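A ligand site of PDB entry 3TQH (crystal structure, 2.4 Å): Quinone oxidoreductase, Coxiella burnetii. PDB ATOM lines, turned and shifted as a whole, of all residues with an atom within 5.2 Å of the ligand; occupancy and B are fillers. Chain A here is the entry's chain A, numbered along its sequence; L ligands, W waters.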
ATOM      1  N   ASN A  46       7.983 -24.995 -21.950  1.00  0.00           N
ATOM      2  CA  ASN A  46       6.673 -25.425 -22.429  1.00  0.00           C
ATOM      3  C   ASN A  46       5.745 -25.603 -21.229  1.00  0.00           C
ATOM      4  O   ASN A  46       6.205 -25.877 -20.124  1.00  0.00           O
ATOM      5  CB  ASN A  46       6.791 -26.744 -23.168  1.00  0.00           C
ATOM      6  CG  ASN A  46       7.649 -26.633 -24.407  1.00  0.00           C
ATOM      7  OD1 ASN A  46       8.872 -26.850 -24.347  1.00  0.00           O
ATOM      8  ND2 ASN A  46       7.029 -26.273 -25.529  1.00  0.00           N
ATOM      9  N   PRO A  47       4.427 -25.444 -21.436  1.00  0.00           N
ATOM     10  CA  PRO A  47       3.460 -25.660 -20.353  1.00  0.00           C
ATOM     11  C   PRO A  47       3.582 -27.001 -19.613  1.00  0.00           C
ATOM     12  O   PRO A  47       3.362 -27.063 -18.388  1.00  0.00           O
ATOM     13  CB  PRO A  47       2.119 -25.552 -21.072  1.00  0.00           C
ATOM     14  CG  PRO A  47       2.384 -24.596 -22.196  1.00  0.00           C
ATOM     15  CD  PRO A  47       3.773 -24.909 -22.649  1.00  0.00           C
ATOM     16  N   ILE A  48       3.903 -28.069 -20.343  1.00  0.00           N
ATOM     17  CA  ILE A  48       4.174 -29.373 -19.740  1.00  0.00           C
ATOM     18  C   ILE A  48       5.154 -29.244 -18.555  1.00  0.00           C
ATOM     19  O   ILE A  48       5.039 -29.979 -17.576  1.00  0.00           O
ATOM     20  CB  ILE A  48       4.701 -30.396 -20.776  1.00  0.00           C
ATOM     21  CG1 ILE A  48       4.714 -31.826 -20.199  1.00  0.00           C
ATOM     22  CG2 ILE A  48       6.087 -30.036 -21.243  1.00  0.00           C
ATOM     23  CD1 ILE A  48       3.413 -32.549 -20.353  1.00  0.00           C
ATOM     24  N   LYS A  51       3.021 -27.994 -15.473  1.00  0.00           N
ATOM     25  CA  LYS A  51       2.061 -29.042 -15.120  1.00  0.00           C
ATOM     26  C   LYS A  51       2.748 -30.216 -14.425  1.00  0.00           C
ATOM     27  O   LYS A  51       2.152 -30.911 -13.594  1.00  0.00           O
ATOM     28  CB  LYS A  51       1.333 -29.555 -16.366  1.00  0.00           C
ATOM     29  CG  LYS A  51       0.500 -28.509 -17.092  1.00  0.00           C
ATOM     30  CD  LYS A  51       0.098 -29.000 -18.470  1.00  0.00           C
ATOM     31  CE  LYS A  51      -0.850 -28.037 -19.168  1.00  0.00           C
ATOM     32  NZ  LYS A  51      -1.463 -28.640 -20.391  1.00  0.00           N
ATOM     33  N   THR A 136       9.501 -28.718 -29.664  1.00  0.00           N
ATOM     34  CA  THR A 136       8.188 -29.122 -29.152  1.00  0.00           C
ATOM     35  C   THR A 136       7.052 -28.363 -29.852  1.00  0.00           C
ATOM     36  O   THR A 136       6.154 -28.973 -30.421  1.00  0.00           O
ATOM     37  CB  THR A 136       8.067 -28.961 -27.614  1.00  0.00           C
ATOM     38  OG1 THR A 136       8.880 -29.962 -26.973  1.00  0.00           O
ATOM     39  CG2 THR A 136       6.619 -29.139 -27.162  1.00  0.00           C
ATOM     40  N   THR A 140       4.621 -30.053 -32.735  1.00  0.00           N
ATOM     41  CA  THR A 140       3.229 -30.190 -32.348  1.00  0.00           C
ATOM     42  C   THR A 140       2.311 -29.491 -33.352  1.00  0.00           C
ATOM     43  O   THR A 140       1.337 -30.074 -33.841  1.00  0.00           O
ATOM     44  CB  THR A 140       2.971 -29.645 -30.939  1.00  0.00           C
ATOM     45  OG1 THR A 140       3.886 -30.244 -30.024  1.00  0.00           O
ATOM     46  CG2 THR A 140       1.552 -29.958 -30.508  1.00  0.00           C
ATOM     47  N   HIS A 159      -7.384 -22.550 -31.822  1.00  0.00           N
ATOM     48  CA  HIS A 159      -7.516 -21.891 -30.529  1.00  0.00           C
ATOM     49  C   HIS A 159      -6.157 -21.510 -29.987  1.00  0.00           C
ATOM     50  O   HIS A 159      -5.161 -22.172 -30.268  1.00  0.00           O
ATOM     51  CB  HIS A 159      -8.220 -22.804 -29.517  1.00  0.00           C
ATOM     52  CG  HIS A 159      -9.699 -22.893 -29.700  1.00  0.00           C
ATOM     53  ND1 HIS A 159     -10.551 -21.853 -29.408  1.00  0.00           N
ATOM     54  CD2 HIS A 159     -10.484 -23.916 -30.121  1.00  0.00           C
ATOM     55  CE1 HIS A 159     -11.795 -22.217 -29.663  1.00  0.00           C
ATOM     56  NE2 HIS A 159     -11.779 -23.472 -30.092  1.00  0.00           N
ATOM     57  N   ALA A 160      -6.114 -20.442 -29.191  1.00  0.00           N
ATOM     58  CA  ALA A 160      -4.879 -20.022 -28.529  1.00  0.00           C
ATOM     59  C   ALA A 160      -3.789 -19.738 -29.548  1.00  0.00           C
ATOM     60  O   ALA A 160      -2.660 -20.206 -29.409  1.00  0.00           O
ATOM     61  CB  ALA A 160      -4.420 -21.083 -27.542  1.00  0.00           C
ATOM     62  N   GLY A 161      -4.134 -18.949 -30.567  1.00  0.00           N
ATOM     63  CA  GLY A 161      -3.244 -18.711 -31.703  1.00  0.00           C
ATOM     64  C   GLY A 161      -1.978 -17.950 -31.403  1.00  0.00           C
ATOM     65  O   GLY A 161      -1.009 -18.064 -32.146  1.00  0.00           O
ATOM     66  N   ALA A 162      -1.959 -17.174 -30.322  1.00  0.00           N
ATOM     67  CA  ALA A 162      -0.826 -16.287 -30.018  1.00  0.00           C
ATOM     68  C   ALA A 162       0.289 -16.996 -29.230  1.00  0.00           C
ATOM     69  O   ALA A 162       1.360 -16.429 -29.055  1.00  0.00           O
ATOM     70  CB  ALA A 162      -1.301 -15.054 -29.254  1.00  0.00           C
ATOM     71  N   GLY A 163       0.038 -18.219 -28.781  1.00  0.00           N
ATOM     72  CA  GLY A 163       0.970 -18.930 -27.909  1.00  0.00           C
ATOM     73  C   GLY A 163       2.053 -19.713 -28.615  1.00  0.00           C
ATOM     74  O   GLY A 163       2.267 -19.563 -29.828  1.00  0.00           O
ATOM     75  N   GLY A 164       2.716 -20.571 -27.860  1.00  0.00           N
ATOM     76  CA  GLY A 164       3.846 -21.348 -28.350  1.00  0.00           C
ATOM     77  C   GLY A 164       3.518 -22.135 -29.596  1.00  0.00           C
ATOM     78  O   GLY A 164       4.085 -21.869 -30.663  1.00  0.00           O
ATOM     79  N   VAL A 165       2.586 -23.080 -29.486  1.00  0.00           N
ATOM     80  CA  VAL A 165       2.207 -23.921 -30.623  1.00  0.00           C
ATOM     81  C   VAL A 165       1.402 -23.117 -31.633  1.00  0.00           C
ATOM     82  O   VAL A 165       1.656 -23.217 -32.828  1.00  0.00           O
ATOM     83  CB  VAL A 165       1.357 -25.131 -30.165  1.00  0.00           C
ATOM     84  CG1 VAL A 165       0.837 -25.913 -31.384  1.00  0.00           C
ATOM     85  CG2 VAL A 165       2.178 -26.036 -29.259  1.00  0.00           C
ATOM     86  N   GLY A 166       0.455 -22.326 -31.143  1.00  0.00           N
ATOM     87  CA  GLY A 166      -0.502 -21.606 -31.979  1.00  0.00           C
ATOM     88  C   GLY A 166       0.104 -20.746 -33.068  1.00  0.00           C
ATOM     89  O   GLY A 166      -0.254 -20.867 -34.245  1.00  0.00           O
ATOM     90  N   THR A 183      -8.540 -17.768 -32.006  1.00  0.00           N
ATOM     91  CA  THR A 183      -9.003 -17.068 -30.815  1.00  0.00           C
ATOM     92  C   THR A 183      -7.820 -16.470 -30.033  1.00  0.00           C
ATOM     93  O   THR A 183      -6.835 -17.152 -29.777  1.00  0.00           O
ATOM     94  CB  THR A 183      -9.825 -17.986 -29.888  1.00  0.00           C
ATOM     95  OG1 THR A 183      -9.114 -19.212 -29.663  1.00  0.00           O
ATOM     96  CG2 THR A 183     -11.177 -18.304 -30.515  1.00  0.00           C
ATOM     97  N   ALA A 184      -7.947 -15.194 -29.669  1.00  0.00           N
ATOM     98  CA  ALA A 184      -6.933 -14.509 -28.871  1.00  0.00           C
ATOM     99  C   ALA A 184      -7.489 -13.232 -28.238  1.00  0.00           C
ATOM    100  O   ALA A 184      -8.579 -12.777 -28.581  1.00  0.00           O
ATOM    101  CB  ALA A 184      -5.746 -14.192 -29.741  1.00  0.00           C
ATOM    102  N   SER A 185      -6.724 -12.655 -27.308  1.00  0.00           N
ATOM    103  CA  SER A 185      -7.027 -11.328 -26.767  1.00  0.00           C
ATOM    104  C   SER A 185      -6.996 -10.265 -27.858  1.00  0.00           C
ATOM    105  O   SER A 185      -6.305 -10.427 -28.868  1.00  0.00           O
ATOM    106  CB  SER A 185      -6.013 -10.938 -25.689  1.00  0.00           C
ATOM    107  OG  SER A 185      -6.094 -11.811 -24.580  1.00  0.00           O
ATOM    108  N   ASN A 188      -3.634  -9.290 -29.055  1.00  0.00           N
ATOM    109  CA  ASN A 188      -2.906 -10.159 -30.000  1.00  0.00           C
ATOM    110  C   ASN A 188      -3.512 -10.204 -31.419  1.00  0.00           C
ATOM    111  O   ASN A 188      -2.967 -10.852 -32.298  1.00  0.00           O
ATOM    112  CB  ASN A 188      -2.798 -11.568 -29.433  1.00  0.00           C
ATOM    113  CG  ASN A 188      -1.923 -11.651 -28.199  1.00  0.00           C
ATOM    114  OD1 ASN A 188      -2.279 -12.289 -27.212  1.00  0.00           O
ATOM    115  ND2 ASN A 188      -0.766 -11.016 -28.245  1.00  0.00           N
ATOM    116  N   TYR A 203     -12.164 -13.783 -27.698  1.00  0.00           N
ATOM    117  CA  TYR A 203     -12.927 -14.779 -26.936  1.00  0.00           C
ATOM    118  C   TYR A 203     -13.416 -14.310 -25.566  1.00  0.00           C
ATOM    119  O   TYR A 203     -14.226 -14.992 -24.936  1.00  0.00           O
ATOM    120  CB  TYR A 203     -12.150 -16.097 -26.808  1.00  0.00           C
ATOM    121  CG  TYR A 203     -10.923 -16.034 -25.925  1.00  0.00           C
ATOM    122  CD1 TYR A 203     -10.975 -16.447 -24.595  1.00  0.00           C
ATOM    123  CD2 TYR A 203      -9.710 -15.573 -26.419  1.00  0.00           C
ATOM    124  CE1 TYR A 203      -9.845 -16.391 -23.785  1.00  0.00           C
ATOM    125  CE2 TYR A 203      -8.582 -15.532 -25.627  1.00  0.00           C
ATOM    126  CZ  TYR A 203      -8.645 -15.938 -24.312  1.00  0.00           C
ATOM    127  OH  TYR A 203      -7.505 -15.877 -23.547  1.00  0.00           O
ATOM    128  N   HIS A 204     -12.951 -13.142 -25.112  1.00  0.00           N
ATOM    129  CA  HIS A 204     -13.478 -12.523 -23.892  1.00  0.00           C
ATOM    130  C   HIS A 204     -14.782 -11.796 -24.127  1.00  0.00           C
ATOM    131  O   HIS A 204     -15.562 -11.591 -23.191  1.00  0.00           O
ATOM    132  CB  HIS A 204     -12.473 -11.519 -23.317  1.00  0.00           C
ATOM    133  CG  HIS A 204     -11.139 -12.101 -23.010  1.00  0.00           C
ATOM    134  ND1 HIS A 204     -10.970 -13.210 -22.217  1.00  0.00           N
ATOM    135  CD2 HIS A 204      -9.893 -11.731 -23.394  1.00  0.00           C
ATOM    136  CE1 HIS A 204      -9.688 -13.502 -22.125  1.00  0.00           C
ATOM    137  NE2 HIS A 204      -9.009 -12.612 -22.826  1.00  0.00           N
ATOM    138  N   LEU A 222      -6.028 -26.051 -28.838  1.00  0.00           N
ATOM    139  CA  LEU A 222      -4.848 -25.958 -27.987  1.00  0.00           C
ATOM    140  C   LEU A 222      -5.193 -25.515 -26.565  1.00  0.00           C
ATOM    141  O   LEU A 222      -4.289 -25.229 -25.786  1.00  0.00           O
ATOM    142  CB  LEU A 222      -3.833 -25.017 -28.619  1.00  0.00           C
ATOM    143  CG  LEU A 222      -3.300 -25.491 -29.983  1.00  0.00           C
ATOM    144  CD1 LEU A 222      -2.619 -24.352 -30.721  1.00  0.00           C
ATOM    145  CD2 LEU A 222      -2.353 -26.685 -29.805  1.00  0.00           C
ATOM    146  N   VAL A 223      -6.491 -25.466 -26.229  1.00  0.00           N
ATOM    147  CA  VAL A 223      -6.943 -25.113 -24.867  1.00  0.00           C
ATOM    148  C   VAL A 223      -7.545 -26.331 -24.140  1.00  0.00           C
ATOM    149  O   VAL A 223      -7.273 -26.543 -22.962  1.00  0.00           O
ATOM    150  CB  VAL A 223      -7.967 -23.958 -24.872  1.00  0.00           C
ATOM    151  CG1 VAL A 223      -8.416 -23.624 -23.454  1.00  0.00           C
ATOM    152  CG2 VAL A 223      -7.373 -22.738 -25.565  1.00  0.00           C
ATOM    153  N   VAL A 227     -13.592 -25.462 -23.831  1.00  0.00           N
ATOM    154  CA  VAL A 227     -13.362 -24.790 -25.117  1.00  0.00           C
ATOM    155  C   VAL A 227     -13.313 -25.809 -26.238  1.00  0.00           C
ATOM    156  O   VAL A 227     -13.916 -25.615 -27.293  1.00  0.00           O
ATOM    157  CB  VAL A 227     -12.065 -23.956 -25.112  1.00  0.00           C
ATOM    158  CG1 VAL A 227     -11.588 -23.691 -26.544  1.00  0.00           C
ATOM    159  CG2 VAL A 227     -12.272 -22.652 -24.365  1.00  0.00           C
ATOM    160  N   VAL A 244      -5.305 -31.033 -28.368  1.00  0.00           N
ATOM    161  CA  VAL A 244      -3.870 -31.223 -28.116  1.00  0.00           C
ATOM    162  C   VAL A 244      -3.487 -31.432 -26.628  1.00  0.00           C
ATOM    163  O   VAL A 244      -2.605 -32.241 -26.345  1.00  0.00           O
ATOM    164  CB  VAL A 244      -3.041 -30.070 -28.750  1.00  0.00           C
ATOM    165  CG1 VAL A 244      -1.567 -30.160 -28.385  1.00  0.00           C
ATOM    166  CG2 VAL A 244      -3.224 -30.077 -30.262  1.00  0.00           C
ATOM    167  N   PRO A 245      -4.124 -30.703 -25.688  1.00  0.00           N
ATOM    168  CA  PRO A 245      -3.823 -31.010 -24.294  1.00  0.00           C
ATOM    169  C   PRO A 245      -4.299 -32.414 -23.942  1.00  0.00           C
ATOM    170  O   PRO A 245      -5.450 -32.763 -24.222  1.00  0.00           O
ATOM    171  CB  PRO A 245      -4.588 -29.946 -23.496  1.00  0.00           C
ATOM    172  CG  PRO A 245      -4.880 -28.864 -24.481  1.00  0.00           C
ATOM    173  CD  PRO A 245      -5.039 -29.550 -25.802  1.00  0.00           C
ATOM    174  N   THR A 246      -3.408 -33.207 -23.359  1.00  0.00           N
ATOM    175  CA  THR A 246      -3.637 -34.631 -23.186  1.00  0.00           C
ATOM    176  C   THR A 246      -4.649 -34.967 -22.101  1.00  0.00           C
ATOM    177  O   THR A 246      -5.340 -35.975 -22.181  1.00  0.00           O
ATOM    178  CB  THR A 246      -2.309 -35.351 -22.849  1.00  0.00           C
ATOM    179  OG1 THR A 246      -1.721 -34.749 -21.698  1.00  0.00           O
ATOM    180  CG2 THR A 246      -1.331 -35.264 -24.031  1.00  0.00           C
ATOM    181  N   LEU A 266      -3.473 -35.831 -29.571  1.00  0.00           N
ATOM    182  CA  LEU A 266      -2.152 -35.698 -30.168  1.00  0.00           C
ATOM    183  C   LEU A 266      -1.093 -35.920 -29.099  1.00  0.00           C
ATOM    184  O   LEU A 266      -1.139 -35.308 -28.032  1.00  0.00           O
ATOM    185  CB  LEU A 266      -1.966 -34.313 -30.781  1.00  0.00           C
ATOM    186  CG  LEU A 266      -0.784 -34.219 -31.759  1.00  0.00           C
ATOM    187  CD1 LEU A 266      -1.213 -34.668 -33.140  1.00  0.00           C
ATOM    188  CD2 LEU A 266      -0.208 -32.806 -31.816  1.00  0.00           C
ATOM    189  N   LEU A 267      -0.153 -36.812 -29.400  1.00  0.00           N
ATOM    190  CA  LEU A 267       1.086 -36.963 -28.633  1.00  0.00           C
ATOM    191  C   LEU A 267       2.245 -36.654 -29.564  1.00  0.00           C
ATOM    192  O   LEU A 267       2.533 -37.417 -30.504  1.00  0.00           O
ATOM    193  CB  LEU A 267       1.220 -38.383 -28.078  1.00  0.00           C
ATOM    194  CG  LEU A 267       0.321 -38.728 -26.885  1.00  0.00           C
ATOM    195  CD1 LEU A 267       0.229 -40.242 -26.719  1.00  0.00           C
ATOM    196  CD2 LEU A 267       0.831 -38.069 -25.602  1.00  0.00           C
ATOM    197  N   LYS A 268       2.893 -35.514 -29.323  1.00  0.00           N
ATOM    198  CA  LYS A 268       4.050 -35.081 -30.099  1.00  0.00           C
ATOM    199  C   LYS A 268       5.117 -36.167 -30.152  1.00  0.00           C
ATOM    200  O   LYS A 268       5.554 -36.658 -29.113  1.00  0.00           O
ATOM    201  CB  LYS A 268       4.640 -33.799 -29.499  1.00  0.00           C
ATOM    202  CG  LYS A 268       5.978 -33.353 -30.132  1.00  0.00           C
ATOM    203  CD  LYS A 268       6.927 -32.770 -29.088  1.00  0.00           C
ATOM    204  CE  LYS A 268       7.526 -33.827 -28.166  1.00  0.00           C
ATOM    205  NZ  LYS A 268       7.885 -33.252 -26.829  1.00  0.00           N
ATOM    206  N   LEU A 307       4.790 -18.064 -17.498  1.00  0.00           N
ATOM    207  CA  LEU A 307       4.269 -19.155 -18.312  1.00  0.00           C
ATOM    208  C   LEU A 307       2.911 -19.676 -17.823  1.00  0.00           C
ATOM    209  O   LEU A 307       2.021 -19.951 -18.635  1.00  0.00           O
ATOM    210  CB  LEU A 307       5.280 -20.302 -18.346  1.00  0.00           C
ATOM    211  CG  LEU A 307       5.060 -21.411 -19.379  1.00  0.00           C
ATOM    212  CD1 LEU A 307       5.269 -20.891 -20.799  1.00  0.00           C
ATOM    213  CD2 LEU A 307       5.981 -22.615 -19.093  1.00  0.00           C
ATOM    214  N   GLY A 310      -0.846 -18.458 -18.662  1.00  0.00           N
ATOM    215  CA  GLY A 310      -1.507 -18.909 -19.882  1.00  0.00           C
ATOM    216  C   GLY A 310      -1.639 -17.808 -20.928  1.00  0.00           C
ATOM    217  O   GLY A 310      -2.398 -17.954 -21.880  1.00  0.00           O
ATOM    218  N   HIS A 311      -0.879 -16.727 -20.780  1.00  0.00           N
ATOM    219  CA  HIS A 311      -0.964 -15.600 -21.707  1.00  0.00           C
ATOM    220  C   HIS A 311       0.378 -15.217 -22.354  1.00  0.00           C
ATOM    221  O   HIS A 311       0.563 -14.088 -22.816  1.00  0.00           O
ATOM    222  CB  HIS A 311      -1.661 -14.427 -21.023  1.00  0.00           C
ATOM    223  CG  HIS A 311      -3.102 -14.682 -20.762  1.00  0.00           C
ATOM    224  ND1 HIS A 311      -3.629 -14.838 -19.500  1.00  0.00           N
ATOM    225  CD2 HIS A 311      -4.135 -14.885 -21.622  1.00  0.00           C
ATOM    226  CE1 HIS A 311      -4.923 -15.089 -19.583  1.00  0.00           C
ATOM    227  NE2 HIS A 311      -5.259 -15.122 -20.860  1.00  0.00           N
ATOM    228  N   VAL A 312       1.298 -16.161 -22.412  1.00  0.00           N
ATOM    229  CA  VAL A 312       2.554 -15.938 -23.109  1.00  0.00           C
ATOM    230  C   VAL A 312       2.296 -15.874 -24.616  1.00  0.00           C
ATOM    231  O   VAL A 312       1.632 -16.749 -25.174  1.00  0.00           O
ATOM    232  CB  VAL A 312       3.598 -17.035 -22.809  1.00  0.00           C
ATOM    233  CG1 VAL A 312       4.817 -16.863 -23.680  1.00  0.00           C
ATOM    234  CG2 VAL A 312       3.982 -16.987 -21.353  1.00  0.00           C
ATOM    235  N   ARG A 313       2.801 -14.828 -25.257  1.00  0.00           N
ATOM    236  CA  ARG A 313       2.815 -14.716 -26.701  1.00  0.00           C
ATOM    237  C   ARG A 313       4.089 -15.395 -27.170  1.00  0.00           C
ATOM    238  O   ARG A 313       5.171 -15.077 -26.668  1.00  0.00           O
ATOM    239  CB  ARG A 313       2.792 -13.252 -27.140  1.00  0.00           C
ATOM    240  CG  ARG A 313       2.739 -13.061 -28.647  1.00  0.00           C
ATOM    241  CD  ARG A 313       3.185 -11.669 -29.072  1.00  0.00           C
ATOM    242  NE  ARG A 313       2.169 -10.659 -28.786  1.00  0.00           N
ATOM    243  CZ  ARG A 313       2.100  -9.474 -29.377  1.00  0.00           C
ATOM    244  NH1 ARG A 313       2.993  -9.112 -30.297  1.00  0.00           N
ATOM    245  NH2 ARG A 313       1.124  -8.630 -29.054  1.00  0.00           N
ATOM    246  N   GLY A 314       3.971 -16.330 -28.107  1.00  0.00           N
ATOM    247  CA  GLY A 314       5.143 -17.063 -28.613  1.00  0.00           C
ATOM    248  C   GLY A 314       5.841 -17.915 -27.568  1.00  0.00           C
ATOM    249  O   GLY A 314       5.197 -18.675 -26.830  1.00  0.00           O
HETATM  250  P1  LIG L   1       1.013 -21.461 -24.381  1.00  0.00           P
HETATM  251  O1  LIG L   1       1.169 -21.222 -22.929  1.00  0.00           O
HETATM  252  O2  LIG L   1       2.187 -20.992 -25.131  1.00  0.00           O
HETATM  253  O3  LIG L   1      -0.295 -20.707 -24.929  1.00  0.00           O
HETATM  254  C1  LIG L   1      -0.596 -19.409 -24.440  1.00  0.00           C
HETATM  255  C2  LIG L   1      -1.682 -18.777 -25.306  1.00  0.00           C
HETATM  256  O4  LIG L   1      -2.940 -19.318 -24.939  1.00  0.00           O
HETATM  257  C3  LIG L   1      -1.807 -17.266 -25.140  1.00  0.00           C
HETATM  258  O5  LIG L   1      -1.313 -16.623 -26.295  1.00  0.00           O
HETATM  259  C4  LIG L   1      -3.290 -17.006 -24.925  1.00  0.00           C
HETATM  260  O6  LIG L   1      -3.808 -16.019 -25.791  1.00  0.00           O
HETATM  261  C5  LIG L   1      -3.927 -18.355 -25.229  1.00  0.00           C
HETATM  262  N1  LIG L   1      -5.133 -18.660 -24.431  1.00  0.00           N
HETATM  263  C6  LIG L   1      -5.201 -18.820 -23.070  1.00  0.00           C
HETATM  264  N2  LIG L   1      -6.484 -19.116 -22.747  1.00  0.00           N
HETATM  265  C7  LIG L   1      -7.218 -19.155 -23.872  1.00  0.00           C
HETATM  266  C8  LIG L   1      -8.565 -19.398 -24.095  1.00  0.00           C
HETATM  267  N3  LIG L   1      -9.357 -19.664 -23.070  1.00  0.00           N
HETATM  268  N4  LIG L   1      -9.069 -19.365 -25.379  1.00  0.00           N
HETATM  269  C9  LIG L   1      -8.212 -19.087 -26.435  1.00  0.00           C
HETATM  270  N5  LIG L   1      -6.870 -18.841 -26.219  1.00  0.00           N
HETATM  271  C10 LIG L   1      -6.378 -18.868 -24.952  1.00  0.00           C
HETATM  272  O7  LIG L   1       0.710 -23.019 -24.663  1.00  0.00           O
HETATM  273  P2  LIG L   1       1.286 -23.906 -25.891  1.00  0.00           P
HETATM  274  O8  LIG L   1       2.711 -24.191 -25.642  1.00  0.00           O
HETATM  275  O9  LIG L   1       0.884 -23.367 -27.199  1.00  0.00           O
HETATM  276  O10 LIG L   1       0.458 -25.261 -25.623  1.00  0.00           O
HETATM  277  C11 LIG L   1      -0.949 -25.280 -25.546  1.00  0.00           C
HETATM  278  C12 LIG L   1      -1.420 -26.574 -24.894  1.00  0.00           C
HETATM  279  O11 LIG L   1      -1.008 -27.686 -25.669  1.00  0.00           O
HETATM  280  C13 LIG L   1      -0.817 -26.749 -23.505  1.00  0.00           C
HETATM  281  O12 LIG L   1      -1.819 -27.170 -22.617  1.00  0.00           O
HETATM  282  C14 LIG L   1       0.260 -27.800 -23.695  1.00  0.00           C
HETATM  283  O13 LIG L   1       0.480 -28.560 -22.519  1.00  0.00           O
HETATM  284  C15 LIG L   1      -0.305 -28.611 -24.865  1.00  0.00           C
HETATM  285  N6  LIG L   1       0.709 -29.327 -25.676  1.00  0.00           N
HETATM  286  C16 LIG L   1       0.498 -30.663 -25.928  1.00  0.00           C
HETATM  287  C17 LIG L   1       1.423 -31.432 -26.628  1.00  0.00           C
HETATM  288  C18 LIG L   1       1.171 -32.890 -26.896  1.00  0.00           C
HETATM  289  O14 LIG L   1       2.153 -33.628 -27.600  1.00  0.00           O
HETATM  290  N7  LIG L   1       0.061 -33.468 -26.458  1.00  0.00           N
HETATM  291  C19 LIG L   1       2.676 -30.773 -27.116  1.00  0.00           C
HETATM  292  C20 LIG L   1       2.841 -29.318 -26.823  1.00  0.00           C
HETATM  293  C21 LIG L   1       1.831 -28.660 -26.115  1.00  0.00           C
HETATM  294  P3  LIG L   1      -4.245 -14.565 -25.245  1.00  0.00           P
HETATM  295  O15 LIG L   1      -4.471 -13.670 -26.430  1.00  0.00           O
HETATM  296  O16 LIG L   1      -3.146 -13.990 -24.382  1.00  0.00           O
HETATM  297  O17 LIG L   1      -5.517 -14.640 -24.441  1.00  0.00           O
HETATM  298  O   HOH W   1      -4.123 -16.823 -28.504  1.00  0.00           O
HETATM  299  O   HOH W   2       1.385 -18.945 -21.274  1.00  0.00           O
HETATM  300  O   HOH W   3      -0.311 -22.384 -20.793  1.00  0.00           O
HETATM  301  O   HOH W   4     -11.292 -19.700 -27.007  1.00  0.00           O
HETATM  302  O   HOH W   5      -0.704 -14.187 -25.382  1.00  0.00           O
HETATM  303  O   HOH W   6       4.287 -26.580 -25.675  1.00  0.00           O
HETATM  304  O   HOH W   7       5.303 -23.003 -25.608  1.00  0.00           O
HETATM  305  O   HOH W   8       4.744 -20.498 -24.840  1.00  0.00           O
HETATM  306  O   HOH W   9      -0.738 -21.632 -28.429  1.00  0.00           O
HETATM  307  O   HOH W  10       3.617 -28.257 -23.363  1.00  0.00           O
HETATM  308  O   HOH W  11       4.066 -31.065 -24.334  1.00  0.00           O
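The backbone carbonyl oxygen (O) of Gly 310 lies close to an oxygen (O4) of the ligand, at 3.4 Å.
Residues that only touch the ligand: Pro 47 (3.3 Å), Thr 136 (3.8 Å), Thr 140 (3.2 Å), Ala 162 (3.3 Å), Thr 183 (3.4 Å), Ala 184 (3.5 Å), Leu 222 (3.3 Å), Val 223 (3.8 Å), Pro 245 (3.96 Å), Thr 246 (3.3 Å), Leu 267 (3.6 Å) and His 311 (3.1 Å).
Hydrophobic or aromatic side chains within 4 Å of the ligand: Pro 47, Ala 160, Ala 162, Val 165, Ala 184, Tyr 203, Val 223, Val 244, Pro 245 and His 311.
Within 4 Å of the ligand: Pro 47, Lys 51, Thr 136, Thr 140, Ala 160, Ala 162, Gly 163, Gly 164, Val 165, Thr 183, Ala 184, Ser 185, Asn 188, Tyr 203, Leu 222, Val 223, Val 244, Pro 245, Thr 246, Leu 266, Leu 267, Lys 268, Gly 310, His 311 and Val 312.
The nearest printed residue that does not touch the ligand is Ile 48 (4.1 Å).
O17 of the ligand is in hydrogen-bond range of OH of Tyr 203 (2.5 Å).
The backbone NH of Ser 185 sits at hydrogen-bond distance from an oxygen (O15) of the ligand.
An oxygen (O17) of the ligand lies within hydrogen-bond range of the side-chain hydroxyl (OG) of Ser 185 (2.9 Å).
The backbone NH (N) of Lys 268 lies within hydrogen-bond range of an oxygen (O14) of the ligand (2.7 Å).
The side-chain amino group (NZ) of Lys 51 sits at hydrogen-bond distance from an oxygen (O12) of the ligand, 2.7 Å away.
The backbone carbonyl oxygen of Leu 266 sits at hydrogen-bond distance from a nitrogen (N7) of the ligand, 2.7 Å away.
The side-chain amide oxygen of Asn 188 lies close to an oxygen (O15) of the ligand (2.7 Å).
An oxygen (O2) of the ligand is in hydrogen-bond range of the backbone NH of Gly 164, 2.8 Å away.
N of Val 165 sits at hydrogen-bond distance from O9 of the ligand (2.9 Å).
The backbone carbonyl oxygen (O) of Val 244 lies within hydrogen-bond range of a nitrogen (N7) of the ligand (2.9 Å).
An oxygen (O5) of the ligand is in hydrogen-bond range of the backbone carbonyl oxygen (O) of Val 312.
The backbone NH (N) of Gly 163 lies within hydrogen-bond range of an oxygen (O5) of the ligand, at 3.2 Å.
A nitrogen (N5) of the ligand sits close to the backbone NH of Ala 160, 3.5 Å away.
A ring nitrogen (NE2) of His 204 sits at hydrogen-bond distance from the side-chain hydroxyl (OG) of Ser 185 (3.5 Å).
NZ of Lys 268 is in hydrogen-bond range of OG1 of Thr 136 (3.4 Å).
The guanidinium group (NE) of Arg 313 sits close to the side-chain amide nitrogen (ND2) of Asn 188 (3.0 Å).
The side-chain hydroxyl of Thr 140 sits at hydrogen-bond distance from the backbone carbonyl oxygen of Thr 136, at 2.6 Å.
The backbone NH of Ala 160 sits at hydrogen-bond distance from the side-chain hydroxyl of Thr 183.
The backbone carbonyl oxygen of Ala 162 is in hydrogen-bond range of the backbone NH of Gly 314, at 2.8 Å.
A ring nitrogen (ND1) of His 159 lies within hydrogen-bond range of the side-chain hydroxyl of Thr 183, at 3.0 Å.
The backbone NH (N) of Gly 161 is in hydrogen-bond range of the backbone carbonyl oxygen (O) of Thr 183, 3.3 Å away.
Water W8 lies within hydrogen-bond range of an oxygen (O2) of the ligand (2.6 Å) and the backbone carbonyl oxygen (O) of Gly 314 (2.7 Å).
Water W9 lies within hydrogen-bond range of the backbone carbonyl oxygen (O) of Ala 160 (2.6 Å), an oxygen (O9) of the ligand (2.7 Å) and the backbone NH (N) of Gly 166 (3.0 Å).
Water W4 lies within hydrogen-bond range of a nitrogen (N4) of the ligand (2.8 Å), a ring nitrogen (ND1) of His 159 (3.3 Å) and the side-chain hydroxyl of Thr 183 (3.5 Å).
Water W1 lies within hydrogen-bond range of O6 of the ligand, N of Ala 162, N of Gly 161 and O of Thr 183.
Water W6 bridges the side-chain amide nitrogen of Asn 46 (2.8 Å) and an oxygen (O8) of the ligand (2.9 Å).
Water W10 lies within hydrogen-bond range of the backbone NH of Ile 48 (3.0 Å) and an oxygen (O13) of the ligand (3.3 Å).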
